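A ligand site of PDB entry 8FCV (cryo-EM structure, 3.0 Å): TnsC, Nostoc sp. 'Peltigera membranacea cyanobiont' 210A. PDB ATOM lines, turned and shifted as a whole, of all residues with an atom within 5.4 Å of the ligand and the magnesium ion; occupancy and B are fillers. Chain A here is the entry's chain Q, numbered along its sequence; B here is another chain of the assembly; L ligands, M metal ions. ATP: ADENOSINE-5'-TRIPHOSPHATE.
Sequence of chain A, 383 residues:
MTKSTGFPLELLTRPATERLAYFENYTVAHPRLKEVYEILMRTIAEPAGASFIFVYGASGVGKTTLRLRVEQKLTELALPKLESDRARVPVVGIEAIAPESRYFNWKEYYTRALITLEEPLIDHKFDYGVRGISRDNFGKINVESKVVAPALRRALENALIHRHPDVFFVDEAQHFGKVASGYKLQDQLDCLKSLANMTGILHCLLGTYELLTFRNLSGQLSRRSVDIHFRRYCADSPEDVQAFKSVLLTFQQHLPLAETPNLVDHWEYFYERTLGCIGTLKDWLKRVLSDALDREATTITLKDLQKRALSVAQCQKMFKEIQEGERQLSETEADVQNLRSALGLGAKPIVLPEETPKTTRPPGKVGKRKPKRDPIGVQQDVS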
ATOM      1  N   GLU A  24      10.003  -8.645 -20.974  1.00  0.00           N
ATOM      2  CA  GLU A  24       8.843  -9.275 -20.328  1.00  0.00           C
ATOM      3  C   GLU A  24       9.027  -9.374 -18.814  1.00  0.00           C
ATOM      4  O   GLU A  24       8.075  -9.117 -18.060  1.00  0.00           O
ATOM      5  CB  GLU A  24       8.556 -10.646 -20.937  1.00  0.00           C
ATOM      6  CG  GLU A  24       9.625 -11.692 -20.775  1.00  0.00           C
ATOM      7  CD  GLU A  24       9.205 -13.055 -21.296  1.00  0.00           C
ATOM      8  OE1 GLU A  24       8.928 -13.172 -22.511  1.00  0.00           O
ATOM      9  OE2 GLU A  24       9.151 -14.007 -20.490  1.00  0.00           O
ATOM     10  N   TYR A  26      10.691  -7.287 -17.159  1.00  0.00           N
ATOM     11  CA  TYR A  26      10.754  -5.915 -16.658  1.00  0.00           C
ATOM     12  C   TYR A  26       9.353  -5.414 -16.341  1.00  0.00           C
ATOM     13  O   TYR A  26       8.433  -5.573 -17.150  1.00  0.00           O
ATOM     14  CB  TYR A  26      11.423  -4.985 -17.672  1.00  0.00           C
ATOM     15  CG  TYR A  26      11.127  -3.529 -17.404  1.00  0.00           C
ATOM     16  CD1 TYR A  26      11.757  -2.855 -16.364  1.00  0.00           C
ATOM     17  CD2 TYR A  26      10.197  -2.833 -18.169  1.00  0.00           C
ATOM     18  CE1 TYR A  26      11.482  -1.523 -16.105  1.00  0.00           C
ATOM     19  CE2 TYR A  26       9.914  -1.503 -17.904  1.00  0.00           C
ATOM     20  CZ  TYR A  26      10.560  -0.851 -16.886  1.00  0.00           C
ATOM     21  OH  TYR A  26      10.285   0.468 -16.632  1.00  0.00           O
ATOM     22  N   THR A  27       9.194  -4.801 -15.173  1.00  0.00           N
ATOM     23  CA  THR A  27       7.945  -4.168 -14.768  1.00  0.00           C
ATOM     24  C   THR A  27       8.257  -2.811 -14.137  1.00  0.00           C
ATOM     25  O   THR A  27       9.320  -2.632 -13.535  1.00  0.00           O
ATOM     26  CB  THR A  27       7.145  -5.044 -13.792  1.00  0.00           C
ATOM     27  OG1 THR A  27       5.825  -4.510 -13.641  1.00  0.00           O
ATOM     28  CG2 THR A  27       7.809  -5.121 -12.435  1.00  0.00           C
ATOM     29  N   VAL A  28       7.353  -1.851 -14.313  1.00  0.00           N
ATOM     30  CA  VAL A  28       7.526  -0.491 -13.830  1.00  0.00           C
ATOM     31  C   VAL A  28       6.550  -0.257 -12.680  1.00  0.00           C
ATOM     32  O   VAL A  28       5.466  -0.856 -12.656  1.00  0.00           O
ATOM     33  CB  VAL A  28       7.334   0.540 -14.946  1.00  0.00           C
ATOM     34  CG1 VAL A  28       5.870   0.634 -15.369  1.00  0.00           C
ATOM     35  CG2 VAL A  28       7.878   1.908 -14.532  1.00  0.00           C
ATOM     36  N   HIS A  30       4.217   2.323 -11.173  1.00  0.00           N
ATOM     37  CA  HIS A  30       3.473   3.561 -11.271  1.00  0.00           C
ATOM     38  C   HIS A  30       2.825   3.898  -9.930  1.00  0.00           C
ATOM     39  O   HIS A  30       2.620   3.008  -9.102  1.00  0.00           O
ATOM     40  CB  HIS A  30       2.431   3.458 -12.397  1.00  0.00           C
ATOM     41  CG  HIS A  30       1.408   2.388 -12.183  1.00  0.00           C
ATOM     42  ND1 HIS A  30       1.257   1.331 -13.049  1.00  0.00           N
ATOM     43  CD2 HIS A  30       0.449   2.230 -11.236  1.00  0.00           C
ATOM     44  CE1 HIS A  30       0.271   0.555 -12.625  1.00  0.00           C
ATOM     45  NE2 HIS A  30      -0.231   1.084 -11.530  1.00  0.00           N
ATOM     46  N   LEU A  33       0.087   1.649  -8.331  1.00  0.00           N
ATOM     47  CA  LEU A  33       0.519   0.305  -7.972  1.00  0.00           C
ATOM     48  C   LEU A  33       1.311   0.313  -6.670  1.00  0.00           C
ATOM     49  O   LEU A  33       1.079  -0.516  -5.786  1.00  0.00           O
ATOM     50  CB  LEU A  33       1.348  -0.307  -9.113  1.00  0.00           C
ATOM     51  CG  LEU A  33       1.853  -1.746  -8.963  1.00  0.00           C
ATOM     52  CD1 LEU A  33       0.821  -2.645  -8.306  1.00  0.00           C
ATOM     53  CD2 LEU A  33       2.243  -2.295 -10.328  1.00  0.00           C
ATOM     54  N   ALA A  58      -9.762  -2.838 -12.459  1.00  0.00           N
ATOM     55  CA  ALA A  58     -10.084  -3.135 -13.849  1.00  0.00           C
ATOM     56  C   ALA A  58      -9.295  -4.340 -14.343  1.00  0.00           C
ATOM     57  O   ALA A  58      -8.326  -4.787 -13.704  1.00  0.00           O
ATOM     58  CB  ALA A  58      -9.801  -1.923 -14.726  1.00  0.00           C
ATOM     59  N   SER A  59      -9.714  -4.881 -15.480  1.00  0.00           N
ATOM     60  CA  SER A  59      -9.001  -5.988 -16.090  1.00  0.00           C
ATOM     61  C   SER A  59      -7.701  -5.480 -16.698  1.00  0.00           C
ATOM     62  O   SER A  59      -7.704  -4.922 -17.795  1.00  0.00           O
ATOM     63  CB  SER A  59      -9.871  -6.666 -17.145  1.00  0.00           C
ATOM     64  OG  SER A  59      -9.335  -7.932 -17.499  1.00  0.00           O
ATOM     65  N   GLY A  60      -6.596  -5.663 -15.983  1.00  0.00           N
ATOM     66  CA  GLY A  60      -5.300  -5.248 -16.456  1.00  0.00           C
ATOM     67  C   GLY A  60      -4.637  -4.121 -15.692  1.00  0.00           C
ATOM     68  O   GLY A  60      -3.614  -3.610 -16.146  1.00  0.00           O
ATOM     69  N   VAL A  61      -5.181  -3.720 -14.538  1.00  0.00           N
ATOM     70  CA  VAL A  61      -4.516  -2.709 -13.722  1.00  0.00           C
ATOM     71  C   VAL A  61      -3.264  -3.247 -13.071  1.00  0.00           C
ATOM     72  O   VAL A  61      -2.400  -2.460 -12.656  1.00  0.00           O
ATOM     73  CB  VAL A  61      -5.470  -2.139 -12.667  1.00  0.00           C
ATOM     74  CG1 VAL A  61      -6.625  -1.423 -13.323  1.00  0.00           C
ATOM     75  CG2 VAL A  61      -5.984  -3.255 -11.769  1.00  0.00           C
ATOM     76  N   GLY A  62      -3.118  -4.565 -12.963  1.00  0.00           N
ATOM     77  CA  GLY A  62      -1.940  -5.150 -12.357  1.00  0.00           C
ATOM     78  C   GLY A  62      -2.232  -5.930 -11.091  1.00  0.00           C
ATOM     79  O   GLY A  62      -1.376  -6.027 -10.203  1.00  0.00           O
ATOM     80  N   LYS A  63      -3.450  -6.464 -10.990  1.00  0.00           N
ATOM     81  CA  LYS A  63      -3.821  -7.229  -9.795  1.00  0.00           C
ATOM     82  C   LYS A  63      -2.927  -8.451  -9.624  1.00  0.00           C
ATOM     83  O   LYS A  63      -2.412  -8.702  -8.532  1.00  0.00           O
ATOM     84  CB  LYS A  63      -5.292  -7.638  -9.883  1.00  0.00           C
ATOM     85  CG  LYS A  63      -6.244  -6.478 -10.100  1.00  0.00           C
ATOM     86  CD  LYS A  63      -7.689  -6.951 -10.214  1.00  0.00           C
ATOM     87  CE  LYS A  63      -7.884  -7.844 -11.436  1.00  0.00           C
ATOM     88  NZ  LYS A  63      -7.918  -7.041 -12.696  1.00  0.00           N
ATOM     89  N   THR A  64      -2.718  -9.209 -10.695  1.00  0.00           N
ATOM     90  CA  THR A  64      -1.881 -10.395 -10.609  1.00  0.00           C
ATOM     91  C   THR A  64      -0.430 -10.027 -10.305  1.00  0.00           C
ATOM     92  O   THR A  64       0.224 -10.693  -9.487  1.00  0.00           O
ATOM     93  CB  THR A  64      -1.962 -11.206 -11.902  1.00  0.00           C
ATOM     94  OG1 THR A  64      -3.299 -11.138 -12.425  1.00  0.00           O
ATOM     95  CG2 THR A  64      -1.594 -12.658 -11.648  1.00  0.00           C
ATOM     96  N   THR A  65       0.091  -8.986 -10.952  1.00  0.00           N
ATOM     97  CA  THR A  65       1.462  -8.563 -10.705  1.00  0.00           C
ATOM     98  C   THR A  65       1.647  -8.113  -9.256  1.00  0.00           C
ATOM     99  O   THR A  65       2.645  -8.446  -8.617  1.00  0.00           O
ATOM    100  CB  THR A  65       1.855  -7.445 -11.666  1.00  0.00           C
ATOM    101  OG1 THR A  65       1.015  -6.305 -11.435  1.00  0.00           O
ATOM    102  CG2 THR A  65       1.688  -7.902 -13.095  1.00  0.00           C
ATOM    103  N   ASP A 171      -7.039 -15.487  -6.034  1.00  0.00           N
ATOM    104  CA  ASP A 171      -7.202 -14.699  -7.246  1.00  0.00           C
ATOM    105  C   ASP A 171      -8.476 -15.095  -7.977  1.00  0.00           C
ATOM    106  O   ASP A 171      -9.010 -16.199  -7.806  1.00  0.00           O
ATOM    107  CB  ASP A 171      -5.988 -14.882  -8.154  1.00  0.00           C
ATOM    108  CG  ASP A 171      -5.662 -13.631  -8.950  1.00  0.00           C
ATOM    109  OD1 ASP A 171      -6.598 -12.852  -9.253  1.00  0.00           O
ATOM    110  OD2 ASP A 171      -4.480 -13.418  -9.270  1.00  0.00           O
ATOM    111  N   GLU A 172      -8.964 -14.173  -8.799  1.00  0.00           N
ATOM    112  CA  GLU A 172     -10.186 -14.351  -9.589  1.00  0.00           C
ATOM    113  C   GLU A 172     -11.368 -14.719  -8.688  1.00  0.00           C
ATOM    114  O   GLU A 172     -12.024 -15.751  -8.859  1.00  0.00           O
ATOM    115  CB  GLU A 172      -9.983 -15.400 -10.688  1.00  0.00           C
ATOM    116  CG  GLU A 172      -8.791 -15.112 -11.594  1.00  0.00           C
ATOM    117  CD  GLU A 172      -9.193 -14.389 -12.860  1.00  0.00           C
ATOM    118  OE1 GLU A 172     -10.019 -13.458 -12.779  1.00  0.00           O
ATOM    119  OE2 GLU A 172      -8.670 -14.742 -13.939  1.00  0.00           O
ATOM    120  N   GLN A 174     -14.171 -13.353  -8.586  1.00  0.00           N
ATOM    121  CA  GLN A 174     -15.466 -13.239  -9.233  1.00  0.00           C
ATOM    122  C   GLN A 174     -16.072 -14.608  -9.529  1.00  0.00           C
ATOM    123  O   GLN A 174     -17.298 -14.748  -9.584  1.00  0.00           O
ATOM    124  CB  GLN A 174     -15.351 -12.428 -10.522  1.00  0.00           C
ATOM    125  CG  GLN A 174     -14.435 -13.031 -11.571  1.00  0.00           C
ATOM    126  CD  GLN A 174     -12.986 -12.642 -11.389  1.00  0.00           C
ATOM    127  OE1 GLN A 174     -12.557 -12.323 -10.282  1.00  0.00           O
ATOM    128  NE2 GLN A 174     -12.221 -12.659 -12.478  1.00  0.00           N
ATOM    129  N   PHE A 251       8.327   3.485 -20.567  1.00  0.00           N
ATOM    130  CA  PHE A 251       8.202   2.304 -21.419  1.00  0.00           C
ATOM    131  C   PHE A 251       8.980   2.483 -22.717  1.00  0.00           C
ATOM    132  O   PHE A 251       9.623   1.545 -23.198  1.00  0.00           O
ATOM    133  CB  PHE A 251       6.736   2.008 -21.696  1.00  0.00           C
ATOM    134  CG  PHE A 251       6.124   1.024 -20.733  1.00  0.00           C
ATOM    135  CD1 PHE A 251       6.883  -0.005 -20.193  1.00  0.00           C
ATOM    136  CD2 PHE A 251       4.791   1.120 -20.370  1.00  0.00           C
ATOM    137  CE1 PHE A 251       6.327  -0.907 -19.307  1.00  0.00           C
ATOM    138  CE2 PHE A 251       4.235   0.218 -19.484  1.00  0.00           C
ATOM    139  CZ  PHE A 251       5.005  -0.797 -18.959  1.00  0.00           C
ATOM    140  N   ILE A 278      -2.453  -0.120 -17.163  1.00  0.00           N
ATOM    141  CA  ILE A 278      -1.028  -0.200 -17.457  1.00  0.00           C
ATOM    142  C   ILE A 278      -0.669  -1.578 -18.020  1.00  0.00           C
ATOM    143  O   ILE A 278       0.203  -1.691 -18.891  1.00  0.00           O
ATOM    144  CB  ILE A 278      -0.215   0.137 -16.189  1.00  0.00           C
ATOM    145  CG1 ILE A 278      -0.498   1.576 -15.769  1.00  0.00           C
ATOM    146  CG2 ILE A 278       1.277  -0.070 -16.438  1.00  0.00           C
ATOM    147  CD1 ILE A 278       0.002   2.608 -16.750  1.00  0.00           C
ATOM    148  N   GLY A 279      -1.320  -2.627 -17.531  1.00  0.00           N
ATOM    149  CA  GLY A 279      -1.052  -3.957 -18.071  1.00  0.00           C
ATOM    150  C   GLY A 279      -1.421  -4.076 -19.541  1.00  0.00           C
ATOM    151  O   GLY A 279      -0.739  -4.754 -20.304  1.00  0.00           O
ATOM    152  N   THR A 280      -2.517  -3.426 -19.944  1.00  0.00           N
ATOM    153  CA  THR A 280      -2.889  -3.418 -21.349  1.00  0.00           C
ATOM    154  C   THR A 280      -1.813  -2.745 -22.190  1.00  0.00           C
ATOM    155  O   THR A 280      -1.437  -3.253 -23.250  1.00  0.00           O
ATOM    156  CB  THR A 280      -4.232  -2.704 -21.538  1.00  0.00           C
ATOM    157  OG1 THR A 280      -5.194  -3.249 -20.622  1.00  0.00           O
ATOM    158  CG2 THR A 280      -4.738  -2.891 -22.958  1.00  0.00           C
ATOM    159  N   LYS A 282       1.338  -2.562 -21.395  1.00  0.00           N
ATOM    160  CA  LYS A 282       2.502  -3.430 -21.386  1.00  0.00           C
ATOM    161  C   LYS A 282       2.381  -4.551 -22.402  1.00  0.00           C
ATOM    162  O   LYS A 282       3.304  -4.815 -23.160  1.00  0.00           O
ATOM    163  CB  LYS A 282       2.707  -4.009 -19.976  1.00  0.00           C
ATOM    164  CG  LYS A 282       3.836  -5.032 -19.894  1.00  0.00           C
ATOM    165  CD  LYS A 282       5.158  -4.436 -20.344  1.00  0.00           C
ATOM    166  CE  LYS A 282       6.307  -5.378 -20.044  1.00  0.00           C
ATOM    167  NZ  LYS A 282       6.443  -5.646 -18.590  1.00  0.00           N
ATOM    168  N   LYS A 286       4.498  -5.114 -25.766  1.00  0.00           N
ATOM    169  CA  LYS A 286       5.192  -6.372 -25.977  1.00  0.00           C
ATOM    170  C   LYS A 286       4.879  -6.950 -27.356  1.00  0.00           C
ATOM    171  O   LYS A 286       5.774  -7.430 -28.058  1.00  0.00           O
ATOM    172  CB  LYS A 286       4.811  -7.370 -24.888  1.00  0.00           C
ATOM    173  CG  LYS A 286       5.448  -8.744 -25.052  1.00  0.00           C
ATOM    174  CD  LYS A 286       4.774  -9.779 -24.167  1.00  0.00           C
ATOM    175  CE  LYS A 286       5.640 -10.136 -22.972  1.00  0.00           C
ATOM    176  NZ  LYS A 286       5.829  -8.972 -22.067  1.00  0.00           N
ATOM    177  N   ASN B 197      -6.050 -20.337 -18.286  1.00  0.00           N
ATOM    178  CA  ASN B 197      -5.298 -19.570 -17.302  1.00  0.00           C
ATOM    179  C   ASN B 197      -4.134 -20.297 -16.657  1.00  0.00           C
ATOM    180  O   ASN B 197      -2.985 -20.114 -17.046  1.00  0.00           O
ATOM    181  CB  ASN B 197      -6.230 -19.123 -16.175  1.00  0.00           C
ATOM    182  CG  ASN B 197      -6.710 -17.695 -16.332  1.00  0.00           C
ATOM    183  OD1 ASN B 197      -5.921 -16.758 -16.218  1.00  0.00           O
ATOM    184  ND2 ASN B 197      -8.003 -17.527 -16.585  1.00  0.00           N
ATOM    185  N   GLN B 220     -13.465  -9.041 -18.856  1.00  0.00           N
ATOM    186  CA  GLN B 220     -12.297  -9.884 -18.622  1.00  0.00           C
ATOM    187  C   GLN B 220     -11.981 -10.734 -19.844  1.00  0.00           C
ATOM    188  O   GLN B 220     -10.821 -10.872 -20.236  1.00  0.00           O
ATOM    189  CB  GLN B 220     -12.532 -10.762 -17.392  1.00  0.00           C
ATOM    190  CG  GLN B 220     -11.944 -10.205 -16.111  1.00  0.00           C
ATOM    191  CD  GLN B 220     -10.465 -10.478 -15.968  1.00  0.00           C
ATOM    192  OE1 GLN B 220      -9.892 -11.247 -16.737  1.00  0.00           O
ATOM    193  NE2 GLN B 220      -9.835  -9.848 -14.992  1.00  0.00           N
ATOM    194  N   ARG B 223     -10.786  -8.251 -22.916  1.00  0.00           N
ATOM    195  CA  ARG B 223      -9.374  -7.885 -22.965  1.00  0.00           C
ATOM    196  C   ARG B 223      -8.511  -9.076 -23.365  1.00  0.00           C
ATOM    197  O   ARG B 223      -7.635  -8.970 -24.240  1.00  0.00           O
ATOM    198  CB  ARG B 223      -8.911  -7.326 -21.624  1.00  0.00           C
ATOM    199  CG  ARG B 223      -7.472  -7.709 -21.299  1.00  0.00           C
ATOM    200  CD  ARG B 223      -6.843  -6.897 -20.204  1.00  0.00           C
ATOM    201  NE  ARG B 223      -5.670  -7.582 -19.675  1.00  0.00           N
ATOM    202  CZ  ARG B 223      -4.542  -6.975 -19.338  1.00  0.00           C
ATOM    203  NH1 ARG B 223      -4.385  -5.678 -19.480  1.00  0.00           N
ATOM    204  NH2 ARG B 223      -3.541  -7.701 -18.839  1.00  0.00           N
ATOM    205  N   ARG B 224      -8.736 -10.222 -22.730  1.00  0.00           N
ATOM    206  CA  ARG B 224      -7.849 -11.374 -22.860  1.00  0.00           C
ATOM    207  C   ARG B 224      -8.058 -12.142 -24.160  1.00  0.00           C
ATOM    208  O   ARG B 224      -7.543 -13.263 -24.288  1.00  0.00           O
ATOM    209  CB  ARG B 224      -8.027 -12.299 -21.660  1.00  0.00           C
ATOM    210  CG  ARG B 224      -7.634 -11.653 -20.335  1.00  0.00           C
ATOM    211  CD  ARG B 224      -7.705 -12.642 -19.195  1.00  0.00           C
ATOM    212  NE  ARG B 224      -6.873 -13.812 -19.429  1.00  0.00           N
ATOM    213  CZ  ARG B 224      -6.726 -14.809 -18.579  1.00  0.00           C
ATOM    214  NH1 ARG B 224      -7.344 -14.824 -17.409  1.00  0.00           N
ATOM    215  NH2 ARG B 224      -5.938 -15.828 -18.903  1.00  0.00           N
HETATM  216  PG  ATP L   1      -6.214 -11.102 -13.784  1.00  0.00           P
HETATM  217  O1G ATP L   1      -5.325 -12.264 -13.529  1.00  0.00           O
HETATM  218  O2G ATP L   1      -6.847 -11.106 -15.185  1.00  0.00           O
HETATM  219  O3G ATP L   1      -7.324 -10.933 -12.739  1.00  0.00           O
HETATM  220  PB  ATP L   1      -5.365  -8.306 -14.408  1.00  0.00           P
HETATM  221  O1B ATP L   1      -5.243  -7.224 -13.406  1.00  0.00           O
HETATM  222  O2B ATP L   1      -6.575  -8.217 -15.333  1.00  0.00           O
HETATM  223  O3B ATP L   1      -5.388  -9.738 -13.727  1.00  0.00           O
HETATM  224  PA  ATP L   1      -2.526  -8.050 -15.194  1.00  0.00           P
HETATM  225  O1A ATP L   1      -2.219  -6.773 -15.873  1.00  0.00           O
HETATM  226  O2A ATP L   1      -2.185  -8.101 -13.713  1.00  0.00           O
HETATM  227  O3A ATP L   1      -4.068  -8.407 -15.329  1.00  0.00           O
HETATM  228  O5' ATP L   1      -1.816  -9.267 -15.916  1.00  0.00           O
HETATM  229  C5' ATP L   1      -0.392  -9.445 -15.832  1.00  0.00           C
HETATM  230  C4' ATP L   1       0.247  -8.956 -17.109  1.00  0.00           C
HETATM  231  O4' ATP L   1       0.205  -7.520 -17.157  1.00  0.00           O
HETATM  232  C3' ATP L   1       1.717  -9.337 -17.293  1.00  0.00           C
HETATM  233  O3' ATP L   1       2.034  -9.518 -18.661  1.00  0.00           O
HETATM  234  C2' ATP L   1       2.435  -8.123 -16.702  1.00  0.00           C
HETATM  235  O2' ATP L   1       3.732  -7.950 -17.255  1.00  0.00           O
HETATM  236  C1' ATP L   1       1.510  -6.986 -17.121  1.00  0.00           C
HETATM  237  N9  ATP L   1       1.522  -5.834 -16.223  1.00  0.00           N
HETATM  238  C8  ATP L   1       0.527  -5.460 -15.361  1.00  0.00           C
HETATM  239  N7  ATP L   1       0.796  -4.375 -14.666  1.00  0.00           N
HETATM  240  C5  ATP L   1       2.066  -4.016 -15.113  1.00  0.00           C
HETATM  241  C6  ATP L   1       2.922  -2.955 -14.772  1.00  0.00           C
HETATM  242  N6  ATP L   1       2.626  -2.022 -13.863  1.00  0.00           N
HETATM  243  N1  ATP L   1       4.120  -2.879 -15.402  1.00  0.00           N
HETATM  244  C2  ATP L   1       4.421  -3.820 -16.309  1.00  0.00           C
HETATM  245  N3  ATP L   1       3.692  -4.861 -16.714  1.00  0.00           N
HETATM  246  C4  ATP L   1       2.522  -4.903 -16.070  1.00  0.00           C
HETATM  247 MG    MG M   1      -3.768 -10.707 -14.372  1.00  0.00          MG
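The backbone NH (N) of Thr 64 is in hydrogen-bond range of an oxygen (O2A) of the ligand (3.3 Å).
O2B of the ligand sits at hydrogen-bond distance from N of Gly 60 (2.6 Å).
N of Lys 63 sits at hydrogen-bond distance from O1B of the ligand.
The side-chain amino group of Lys 63 is in salt-bridge range of an oxygen (O1B) of the ligand (2.8 Å).
The side-chain hydroxyl (OG1) of Thr 27 is in hydrogen-bond range of a nitrogen (N1) of the ligand, 2.9 Å away.
N3 of the ligand sits close to NZ of Lys 282, 3.4 Å away.
The side-chain amide nitrogen (NE2) of Gln 220 of chain B sits at hydrogen-bond distance from an oxygen (O2G) of the ligand (3.2 Å).
The backbone NH of Gly 62 is in hydrogen-bond range of an oxygen (O1B) of the ligand.
A nitrogen (N6) of the ligand sits at hydrogen-bond distance from the backbone carbonyl oxygen (O) of Val 28 (3.3 Å).
The guanidinium group (NH2) of Arg 223 of chain B lies within salt-bridge range of an oxygen (O1A) of the ligand.
The backbone carbonyl oxygen (O) of Gly 60 sits at hydrogen-bond distance from the backbone NH (N) of Gly 279, 2.9 Å away.
The backbone carbonyl oxygen of Ala 58 lies within hydrogen-bond range of the side-chain amino group of Lys 63, 2.5 Å away.
The side-chain amino group (NZ) of Lys 282 is in hydrogen-bond range of the backbone carbonyl oxygen (O) of Tyr 26 (2.5 Å).
OG of Ser 59 sits close to NE2 of Gln 220 of chain B (3.2 Å).
The backbone carbonyl oxygen (O) of Gly 62 sits at hydrogen-bond distance from the side-chain hydroxyl (OG1) of Thr 65, at 2.7 Å.
The guanidinium group of Arg 223 of chain B is in hydrogen-bond range of the side-chain hydroxyl of Thr 280, 2.8 Å away.
A ring nitrogen (NE2) of His 30 sits close to the backbone NH (N) of Leu 33, at 3.3 Å.
The guanidinium group (NH1) of Arg 224 of chain B is in salt-bridge range of the side-chain carboxylate (OE2) of Glu 172 (3.7 Å).
Merely in contact with the ligand: His 30, Leu 33, Ala 58, Ser 59, Val 61, Thr 65, Glu 172, Ile 278 and Gly 279.
Hydrophobic or aromatic side chains within 4 Å of the ligand: Val 28, His 30, Leu 33 and Ile 278.
Within 4 Å of the ligand: Thr 27, Val 28, His 30, Leu 33, Ala 58, Ser 59, Gly 60, Val 61, Gly 62, Lys 63, Thr 64, Thr 65, Glu 172, Ile 278, Gly 279, Lys 282, Gln 220 of chain B and Arg 223 of chain B.
The nearest printed residue that does not touch the ligand is Asp 171 (4.04 Å).
Within 4 Å of the magnesium ion: Thr 64.
O3B of the ligand is bound to the magnesium ion.
The side-chain hydroxyl (OG1) of Thr 64 binds the magnesium ion (2.0 Å).
O1G of the ligand binds the magnesium ion (2.4 Å).
The magnesium ion is bound by an oxygen (O3A) of the ligand (2.5 Å).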
